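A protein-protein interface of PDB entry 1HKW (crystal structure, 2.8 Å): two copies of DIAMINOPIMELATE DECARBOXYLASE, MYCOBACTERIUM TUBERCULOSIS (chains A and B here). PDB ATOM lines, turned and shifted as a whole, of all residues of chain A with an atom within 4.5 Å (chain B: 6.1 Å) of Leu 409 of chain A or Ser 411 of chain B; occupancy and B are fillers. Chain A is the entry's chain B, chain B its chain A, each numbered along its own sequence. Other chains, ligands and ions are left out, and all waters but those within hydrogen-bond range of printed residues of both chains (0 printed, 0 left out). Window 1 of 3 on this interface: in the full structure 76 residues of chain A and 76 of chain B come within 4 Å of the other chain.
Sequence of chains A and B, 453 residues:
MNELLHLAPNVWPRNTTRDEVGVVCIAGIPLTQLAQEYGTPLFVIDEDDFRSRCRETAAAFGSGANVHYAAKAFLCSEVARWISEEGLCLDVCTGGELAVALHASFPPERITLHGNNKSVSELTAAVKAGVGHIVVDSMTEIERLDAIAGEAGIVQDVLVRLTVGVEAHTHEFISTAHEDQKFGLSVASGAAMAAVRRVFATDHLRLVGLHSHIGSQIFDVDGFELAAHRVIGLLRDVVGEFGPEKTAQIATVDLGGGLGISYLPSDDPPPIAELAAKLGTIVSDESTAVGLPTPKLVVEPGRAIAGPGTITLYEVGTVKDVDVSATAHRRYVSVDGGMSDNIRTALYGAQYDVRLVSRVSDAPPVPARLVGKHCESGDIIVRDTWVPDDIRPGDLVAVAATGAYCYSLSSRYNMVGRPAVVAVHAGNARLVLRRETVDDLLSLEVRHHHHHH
The side-chain hydroxyl (OH) of Tyr 348 of chain A sits at hydrogen-bond distance from the side-chain carboxylate (OE1) of Glu 376 of chain B.
The backbone carbonyl oxygen (O) of Ser 340 of chain B sits at hydrogen-bond distance from the backbone NH (N) of Ser 411 of chain B (3.2 Å).
A ring nitrogen (ND1) of His 374 of chain B lies close to the backbone carbonyl oxygen (O) of Tyr 413 of chain B.
The side-chain hydroxyl (OH) of Tyr 413 of chain B sits at hydrogen-bond distance from the side-chain carboxylate (OE1) of Glu 376 of chain B (2.7 Å).
OG of Ser 410 of chain B lies within hydrogen-bond range of O of Tyr 407 of chain B.
The side-chain carboxylate (OE2) of Glu 436 of chain B lies within salt-bridge range of the guanidinium group (NH2) of Arg 412 of chain B, at 2.8 Å.
The side-chain hydroxyl of Ser 410 of chain A is in hydrogen-bond range of the backbone carbonyl oxygen of Tyr 407 of chain A (2.5 Å).
Among the printed residues, merely in contact across the chains: Tyr 405 of chain A with Tyr 413 of chain B (3.5 Å), Ser 408 of chain A with Arg 412 of chain B (3.8 Å), Ser 408 of chain A with Tyr 413 of chain B (3.5 Å), Leu 409 of chain A with Met 339 of chain B (3.8 Å), Leu 409 of chain A with Ser 411 of chain B (3.5 Å), Leu 409 of chain A with Tyr 413 of chain B (3.6 Å), Ser 410 of chain A with Ser 411 of chain B (3.1 Å), Ser 411 of chain A with Leu 409 of chain B (3.6 Å) and Ser 411 of chain A with Ser 410 of chain B (3.4 Å).
Tyr 407 of chain A touches none of the printed residues of chain B.
Of the printed residues of chain B, Leu 409 of chain A touches Met 339 (3.8 Å), Ser 411 (3.5 Å) and Tyr 413 (3.6 Å).
Printed residues of chain B within 4 Å of Ser 410 of chain A: Ser 411.
Printed residues of chain A within 4 Å of Met 339 of chain B: Leu 409.
His 374 of chain B touches none of the printed residues of chain A.
Printed residues of chain A within 4 Å of Ser 410 of chain B: Ser 411 (3.4 Å).
Ser 411 of chain B touches two residues of chain A.
The nearest residue of chain B that does not touch Leu 409 of chain A is Glu 376 of chain B (5.0 Å).
The nearest residue of chain A that does not touch Ser 411 of chain B is Ser 408 of chain A (4.4 Å).
The nearest printed residue of chain B that does not touch Ser 411 of chain A is Ser 411 of chain B (4.7 Å).
Printed residues of chain A that touch a printed residue of chain B: Tyr 348, Tyr 405, Ser 408, Leu 409, Ser 410 and Ser 411.
Of the 16 printed residues of chain B, 7 touch a printed residue of chain A.
Among the printed residues, 10 pairs touch across the chains.
Among the printed residues, no Asp or Glu carboxylate lies within 4 Å of a Lys or Arg side-chain nitrogen of the other chain.
Leu 409 of chain A touches Ser 411 of chain B, and with the chains exchanged Ser 411 of chain A touches Leu 409 of chain B.
Ser 410 of chain A touches Ser 411 of chain B, and with the chains exchanged Ser 411 of chain A touches Ser 410 of chain B.
5 positions are printed for both chains.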
ATOM      1  N   ILE A 343       6.084  -5.374   6.676  1.00  0.00           N
ATOM      2  CA  ILE A 343       4.867  -6.009   6.251  1.00  0.00           C
ATOM      3  C   ILE A 343       4.559  -5.652   4.837  1.00  0.00           C
ATOM      4  O   ILE A 343       3.651  -6.237   4.223  1.00  0.00           O
ATOM      5  CB  ILE A 343       3.706  -5.641   7.171  1.00  0.00           C
ATOM      6  CG1 ILE A 343       2.583  -6.646   6.977  1.00  0.00           C
ATOM      7  CG2 ILE A 343       3.253  -4.202   6.912  1.00  0.00           C
ATOM      8  CD1 ILE A 343       1.652  -6.709   8.074  1.00  0.00           C
ATOM      9  N   TYR A 348       1.495  -4.897   0.358  1.00  0.00           N
ATOM     10  CA  TYR A 348       1.472  -4.163  -0.931  1.00  0.00           C
ATOM     11  C   TYR A 348       2.091  -4.953  -2.069  1.00  0.00           C
ATOM     12  O   TYR A 348       2.039  -4.499  -3.206  1.00  0.00           O
ATOM     13  CB  TYR A 348       2.254  -2.855  -0.816  1.00  0.00           C
ATOM     14  CG  TYR A 348       1.844  -1.940   0.326  1.00  0.00           C
ATOM     15  CD1 TYR A 348       2.775  -1.582   1.315  1.00  0.00           C
ATOM     16  CD2 TYR A 348       0.541  -1.416   0.413  1.00  0.00           C
ATOM     17  CE1 TYR A 348       2.433  -0.749   2.347  1.00  0.00           C
ATOM     18  CE2 TYR A 348       0.182  -0.556   1.456  1.00  0.00           C
ATOM     19  CZ  TYR A 348       1.135  -0.228   2.421  1.00  0.00           C
ATOM     20  OH  TYR A 348       0.841   0.595   3.434  1.00  0.00           O
ATOM     21  N   TYR A 405       8.000   3.241   6.098  1.00  0.00           N
ATOM     22  CA  TYR A 405       6.805   2.463   6.285  1.00  0.00           C
ATOM     23  C   TYR A 405       7.004   1.158   6.983  1.00  0.00           C
ATOM     24  O   TYR A 405       6.075   0.667   7.592  1.00  0.00           O
ATOM     25  CB  TYR A 405       5.979   2.348   5.007  1.00  0.00           C
ATOM     26  CG  TYR A 405       5.530   3.722   4.537  1.00  0.00           C
ATOM     27  CD1 TYR A 405       4.478   4.392   5.148  1.00  0.00           C
ATOM     28  CD2 TYR A 405       6.224   4.378   3.530  1.00  0.00           C
ATOM     29  CE1 TYR A 405       4.113   5.695   4.715  1.00  0.00           C
ATOM     30  CE2 TYR A 405       5.885   5.631   3.122  1.00  0.00           C
ATOM     31  CZ  TYR A 405       4.840   6.298   3.702  1.00  0.00           C
ATOM     32  OH  TYR A 405       4.540   7.561   3.231  1.00  0.00           O
ATOM     33  N   CYS A 406       8.217   0.629   7.005  1.00  0.00           N
ATOM     34  CA  CYS A 406       8.459  -0.622   7.746  1.00  0.00           C
ATOM     35  C   CYS A 406       8.280  -0.502   9.258  1.00  0.00           C
ATOM     36  O   CYS A 406       7.406  -1.163   9.813  1.00  0.00           O
ATOM     37  CB  CYS A 406       9.814  -1.162   7.402  1.00  0.00           C
ATOM     38  SG  CYS A 406       9.906  -1.474   5.666  1.00  0.00           S
ATOM     39  N   TYR A 407       9.073   0.344   9.925  1.00  0.00           N
ATOM     40  CA  TYR A 407       8.941   0.468  11.391  1.00  0.00           C
ATOM     41  C   TYR A 407       7.523   1.042  11.848  1.00  0.00           C
ATOM     42  O   TYR A 407       6.975   0.571  12.828  1.00  0.00           O
ATOM     43  CB  TYR A 407      10.090   1.286  11.994  1.00  0.00           C
ATOM     44  CG  TYR A 407      10.047   1.347  13.510  1.00  0.00           C
ATOM     45  CD1 TYR A 407       9.197   2.206  14.174  1.00  0.00           C
ATOM     46  CD2 TYR A 407      10.855   0.536  14.288  1.00  0.00           C
ATOM     47  CE1 TYR A 407       9.153   2.252  15.625  1.00  0.00           C
ATOM     48  CE2 TYR A 407      10.815   0.581  15.717  1.00  0.00           C
ATOM     49  CZ  TYR A 407       9.966   1.438  16.352  1.00  0.00           C
ATOM     50  OH  TYR A 407       9.921   1.467  17.706  1.00  0.00           O
ATOM     51  N   SER A 408       6.962   2.040  11.105  1.00  0.00           N
ATOM     52  CA  SER A 408       5.637   2.654  11.476  1.00  0.00           C
ATOM     53  C   SER A 408       4.529   1.679  11.378  1.00  0.00           C
ATOM     54  O   SER A 408       3.510   1.819  12.095  1.00  0.00           O
ATOM     55  CB  SER A 408       5.231   3.885  10.618  1.00  0.00           C
ATOM     56  OG  SER A 408       6.225   4.274   9.715  1.00  0.00           O
ATOM     57  N   LEU A 409       4.683   0.695  10.489  1.00  0.00           N
ATOM     58  CA  LEU A 409       3.705  -0.380  10.412  1.00  0.00           C
ATOM     59  C   LEU A 409       3.983  -1.542  11.316  1.00  0.00           C
ATOM     60  O   LEU A 409       3.208  -2.468  11.350  1.00  0.00           O
ATOM     61  CB  LEU A 409       3.522  -0.865   8.983  1.00  0.00           C
ATOM     62  CG  LEU A 409       2.851   0.191   8.092  1.00  0.00           C
ATOM     63  CD1 LEU A 409       3.133  -0.065   6.585  1.00  0.00           C
ATOM     64  CD2 LEU A 409       1.355   0.266   8.385  1.00  0.00           C
ATOM     65  N   SER A 410       5.064  -1.518  12.066  1.00  0.00           N
ATOM     66  CA  SER A 410       5.406  -2.700  12.876  1.00  0.00           C
ATOM     67  C   SER A 410       4.273  -3.118  13.777  1.00  0.00           C
ATOM     68  O   SER A 410       3.449  -2.317  14.114  1.00  0.00           O
ATOM     69  CB  SER A 410       6.552  -2.415  13.718  1.00  0.00           C
ATOM     70  OG  SER A 410       6.326  -1.248  14.342  1.00  0.00           O
ATOM     71  N   SER A 411       4.263  -4.381  14.156  1.00  0.00           N
ATOM     72  CA  SER A 411       3.242  -4.952  14.957  1.00  0.00           C
ATOM     73  C   SER A 411       3.880  -5.876  16.107  1.00  0.00           C
ATOM     74  O   SER A 411       5.095  -5.960  16.257  1.00  0.00           O
ATOM     75  CB  SER A 411       2.252  -5.712  14.044  1.00  0.00           C
ATOM     76  OG  SER A 411       2.615  -7.069  13.821  1.00  0.00           O
ATOM     77  N   MET B 339      -6.716   0.622   9.799  1.00  0.00           N
ATOM     78  CA  MET B 339      -5.803  -0.549   9.564  1.00  0.00           C
ATOM     79  C   MET B 339      -4.811  -0.788  10.729  1.00  0.00           C
ATOM     80  O   MET B 339      -4.199  -1.847  10.858  1.00  0.00           O
ATOM     81  CB  MET B 339      -5.051  -0.366   8.237  1.00  0.00           C
ATOM     82  CG  MET B 339      -4.273   0.838   8.184  1.00  0.00           C
ATOM     83  SD  MET B 339      -3.489   1.240   6.413  1.00  0.00           S
ATOM     84  CE  MET B 339      -1.965   0.114   6.443  1.00  0.00           C
ATOM     85  N   SER B 340      -4.683   0.222  11.567  1.00  0.00           N
ATOM     86  CA  SER B 340      -4.031   0.094  12.853  1.00  0.00           C
ATOM     87  C   SER B 340      -4.690  -0.933  13.755  1.00  0.00           C
ATOM     88  O   SER B 340      -4.053  -1.403  14.631  1.00  0.00           O
ATOM     89  CB  SER B 340      -4.025   1.455  13.560  1.00  0.00           C
ATOM     90  OG  SER B 340      -5.373   1.956  13.749  1.00  0.00           O
ATOM     91  N   ASP B 341      -5.972  -1.252  13.558  1.00  0.00           N
ATOM     92  CA  ASP B 341      -6.654  -2.223  14.449  1.00  0.00           C
ATOM     93  C   ASP B 341      -7.430  -3.312  13.757  1.00  0.00           C
ATOM     94  O   ASP B 341      -7.877  -4.216  14.372  1.00  0.00           O
ATOM     95  CB  ASP B 341      -7.578  -1.516  15.483  1.00  0.00           C
ATOM     96  CG  ASP B 341      -8.676  -0.566  14.831  1.00  0.00           C
ATOM     97  OD1 ASP B 341      -8.433   0.707  14.804  1.00  0.00           O
ATOM     98  OD2 ASP B 341      -9.789  -0.992  14.428  1.00  0.00           O
ATOM     99  N   ILE B 343      -6.244  -4.777  10.146  1.00  0.00           N
ATOM    100  CA  ILE B 343      -5.494  -4.654   8.896  1.00  0.00           C
ATOM    101  C   ILE B 343      -5.886  -5.746   7.940  1.00  0.00           C
ATOM    102  O   ILE B 343      -5.503  -5.718   6.809  1.00  0.00           O
ATOM    103  CB  ILE B 343      -3.974  -4.668   9.141  1.00  0.00           C
ATOM    104  CG1 ILE B 343      -3.257  -4.201   7.890  1.00  0.00           C
ATOM    105  CG2 ILE B 343      -3.487  -6.089   9.552  1.00  0.00           C
ATOM    106  CD1 ILE B 343      -1.963  -3.571   8.137  1.00  0.00           C
ATOM    107  N   HIS B 374      -6.340   6.874   8.857  1.00  0.00           N
ATOM    108  CA  HIS B 374      -4.912   6.978   8.466  1.00  0.00           C
ATOM    109  C   HIS B 374      -4.677   7.609   7.103  1.00  0.00           C
ATOM    110  O   HIS B 374      -5.588   7.630   6.292  1.00  0.00           O
ATOM    111  CB  HIS B 374      -4.338   5.614   8.419  1.00  0.00           C
ATOM    112  CG  HIS B 374      -4.375   4.907   9.707  1.00  0.00           C
ATOM    113  ND1 HIS B 374      -3.452   5.139  10.696  1.00  0.00           N
ATOM    114  CD2 HIS B 374      -5.206   3.947  10.174  1.00  0.00           C
ATOM    115  CE1 HIS B 374      -3.715   4.349  11.725  1.00  0.00           C
ATOM    116  NE2 HIS B 374      -4.779   3.620  11.437  1.00  0.00           N
ATOM    117  N   GLU B 376      -3.661   6.926   4.152  1.00  0.00           N
ATOM    118  CA  GLU B 376      -3.425   6.017   3.083  1.00  0.00           C
ATOM    119  C   GLU B 376      -4.750   5.710   2.486  1.00  0.00           C
ATOM    120  O   GLU B 376      -5.715   5.429   3.200  1.00  0.00           O
ATOM    121  CB  GLU B 376      -2.831   4.748   3.634  1.00  0.00           C
ATOM    122  CG  GLU B 376      -1.612   4.249   2.924  1.00  0.00           C
ATOM    123  CD  GLU B 376      -1.192   2.920   3.503  1.00  0.00           C
ATOM    124  OE1 GLU B 376      -0.232   2.930   4.340  1.00  0.00           O
ATOM    125  OE2 GLU B 376      -1.827   1.875   3.156  1.00  0.00           O
ATOM    126  N   TYR B 407      -6.353  -7.690  16.717  1.00  0.00           N
ATOM    127  CA  TYR B 407      -5.619  -6.981  17.752  1.00  0.00           C
ATOM    128  C   TYR B 407      -4.176  -7.442  17.713  1.00  0.00           C
ATOM    129  O   TYR B 407      -3.212  -6.629  17.943  1.00  0.00           O
ATOM    130  CB  TYR B 407      -6.229  -7.249  19.147  1.00  0.00           C
ATOM    131  CG  TYR B 407      -5.501  -6.512  20.255  1.00  0.00           C
ATOM    132  CD1 TYR B 407      -4.393  -7.079  20.900  1.00  0.00           C
ATOM    133  CD2 TYR B 407      -5.882  -5.257  20.619  1.00  0.00           C
ATOM    134  CE1 TYR B 407      -3.684  -6.366  21.900  1.00  0.00           C
ATOM    135  CE2 TYR B 407      -5.194  -4.554  21.604  1.00  0.00           C
ATOM    136  CZ  TYR B 407      -4.106  -5.120  22.243  1.00  0.00           C
ATOM    137  OH  TYR B 407      -3.476  -4.400  23.193  1.00  0.00           O
ATOM    138  N   LEU B 409      -2.578  -8.199  15.242  1.00  0.00           N
ATOM    139  CA  LEU B 409      -1.878  -7.606  14.110  1.00  0.00           C
ATOM    140  C   LEU B 409      -1.741  -6.087  14.208  1.00  0.00           C
ATOM    141  O   LEU B 409      -1.242  -5.442  13.274  1.00  0.00           O
ATOM    142  CB  LEU B 409      -2.566  -7.996  12.801  1.00  0.00           C
ATOM    143  CG  LEU B 409      -2.216  -9.427  12.318  1.00  0.00           C
ATOM    144  CD1 LEU B 409      -3.120  -9.904  11.220  1.00  0.00           C
ATOM    145  CD2 LEU B 409      -0.779  -9.488  11.860  1.00  0.00           C
ATOM    146  N   SER B 410      -2.192  -5.513  15.317  1.00  0.00           N
ATOM    147  CA  SER B 410      -2.337  -4.073  15.388  1.00  0.00           C
ATOM    148  C   SER B 410      -1.001  -3.437  15.389  1.00  0.00           C
ATOM    149  O   SER B 410      -0.011  -4.033  15.910  1.00  0.00           O
ATOM    150  CB  SER B 410      -3.052  -3.664  16.662  1.00  0.00           C
ATOM    151  OG  SER B 410      -2.402  -4.217  17.796  1.00  0.00           O
ATOM    152  N   SER B 411      -0.980  -2.216  14.854  1.00  0.00           N
ATOM    153  CA  SER B 411       0.179  -1.375  14.781  1.00  0.00           C
ATOM    154  C   SER B 411      -0.124   0.021  15.412  1.00  0.00           C
ATOM    155  O   SER B 411      -1.182   0.235  15.969  1.00  0.00           O
ATOM    156  CB  SER B 411       0.620  -1.219  13.312  1.00  0.00           C
ATOM    157  OG  SER B 411      -0.429  -0.701  12.506  1.00  0.00           O
ATOM    158  N   ARG B 412       0.848   0.924  15.336  1.00  0.00           N
ATOM    159  CA  ARG B 412       0.702   2.303  15.759  1.00  0.00           C
ATOM    160  C   ARG B 412       0.952   3.162  14.581  1.00  0.00           C
ATOM    161  O   ARG B 412       1.753   4.020  14.622  1.00  0.00           O
ATOM    162  CB  ARG B 412       1.740   2.640  16.808  1.00  0.00           C
ATOM    163  CG  ARG B 412       1.691   1.756  18.063  1.00  0.00           C
ATOM    164  CD  ARG B 412       2.763   2.139  19.000  1.00  0.00           C
ATOM    165  NE  ARG B 412       2.577   1.642  20.371  1.00  0.00           N
ATOM    166  CZ  ARG B 412       3.591   1.544  21.224  1.00  0.00           C
ATOM    167  NH1 ARG B 412       4.812   1.874  20.851  1.00  0.00           N
ATOM    168  NH2 ARG B 412       3.409   1.084  22.416  1.00  0.00           N
ATOM    169  N   TYR B 413       0.267   2.879  13.503  1.00  0.00           N
ATOM    170  CA  TYR B 413       0.454   3.590  12.281  1.00  0.00           C
ATOM    171  C   TYR B 413      -0.044   5.011  12.496  1.00  0.00           C
ATOM    172  O   TYR B 413      -1.068   5.224  13.144  1.00  0.00           O
ATOM    173  CB  TYR B 413      -0.318   2.851  11.114  1.00  0.00           C
ATOM    174  CG  TYR B 413       0.038   3.348   9.721  1.00  0.00           C
ATOM    175  CD1 TYR B 413      -0.853   3.261   8.702  1.00  0.00           C
ATOM    176  CD2 TYR B 413       1.281   3.918   9.450  1.00  0.00           C
ATOM    177  CE1 TYR B 413      -0.537   3.724   7.412  1.00  0.00           C
ATOM    178  CE2 TYR B 413       1.605   4.387   8.171  1.00  0.00           C
ATOM    179  CZ  TYR B 413       0.683   4.286   7.171  1.00  0.00           C
ATOM    180  OH  TYR B 413       0.958   4.721   5.917  1.00  0.00           O
ATOM    181  N   VAL B 416      -1.252   5.953  16.133  1.00  0.00           N
ATOM    182  CA  VAL B 416      -2.531   5.599  16.715  1.00  0.00           C
ATOM    183  C   VAL B 416      -2.357   4.399  17.644  1.00  0.00           C
ATOM    184  O   VAL B 416      -1.873   3.328  17.236  1.00  0.00           O
ATOM    185  CB  VAL B 416      -3.590   5.263  15.636  1.00  0.00           C
ATOM    186  CG1 VAL B 416      -4.930   4.857  16.282  1.00  0.00           C
ATOM    187  CG2 VAL B 416      -3.794   6.412  14.777  1.00  0.00           C
ATOM    188  N   GLY B 417      -2.780   4.568  18.884  1.00  0.00           N
ATOM    189  CA  GLY B 417      -2.471   3.634  19.911  1.00  0.00           C
ATOM    190  C   GLY B 417      -3.462   2.546  19.905  1.00  0.00           C
ATOM    191  O   GLY B 417      -4.563   2.690  19.372  1.00  0.00           O
ATOM    192  N   ARG B 418      -3.074   1.431  20.512  1.00  0.00           N
ATOM    193  CA  ARG B 418      -3.902   0.279  20.504  1.00  0.00           C
ATOM    194  C   ARG B 418      -5.171   0.611  21.257  1.00  0.00           C
ATOM    195  O   ARG B 418      -5.136   1.185  22.331  1.00  0.00           O
ATOM    196  CB  ARG B 418      -3.166  -0.931  21.100  1.00  0.00           C
ATOM    197  CG  ARG B 418      -2.171  -1.533  20.136  1.00  0.00           C
ATOM    198  CD  ARG B 418      -1.519  -2.872  20.588  1.00  0.00           C
ATOM    199  NE  ARG B 418      -0.079  -2.658  20.812  1.00  0.00           N
ATOM    200  CZ  ARG B 418       0.876  -2.570  19.845  1.00  0.00           C
ATOM    201  NH1 ARG B 418       2.128  -2.317  20.215  1.00  0.00           N
ATOM    202  NH2 ARG B 418       0.591  -2.753  18.536  1.00  0.00           N
ATOM    203  N   GLU B 436      -3.586   2.660  24.676  1.00  0.00           N
ATOM    204  CA  GLU B 436      -2.275   3.309  24.629  1.00  0.00           C
ATOM    205  C   GLU B 436      -2.458   4.777  24.651  1.00  0.00           C
ATOM    206  O   GLU B 436      -3.516   5.245  24.414  1.00  0.00           O
ATOM    207  CB  GLU B 436      -1.413   2.833  23.408  1.00  0.00           C
ATOM    208  CG  GLU B 436      -0.868   1.367  23.578  1.00  0.00           C
ATOM    209  CD  GLU B 436       0.010   0.806  22.402  1.00  0.00           C
ATOM    210  OE1 GLU B 436      -0.167   1.198  21.197  1.00  0.00           O
ATOM    211  OE2 GLU B 436       0.883  -0.077  22.700  1.00  0.00           O
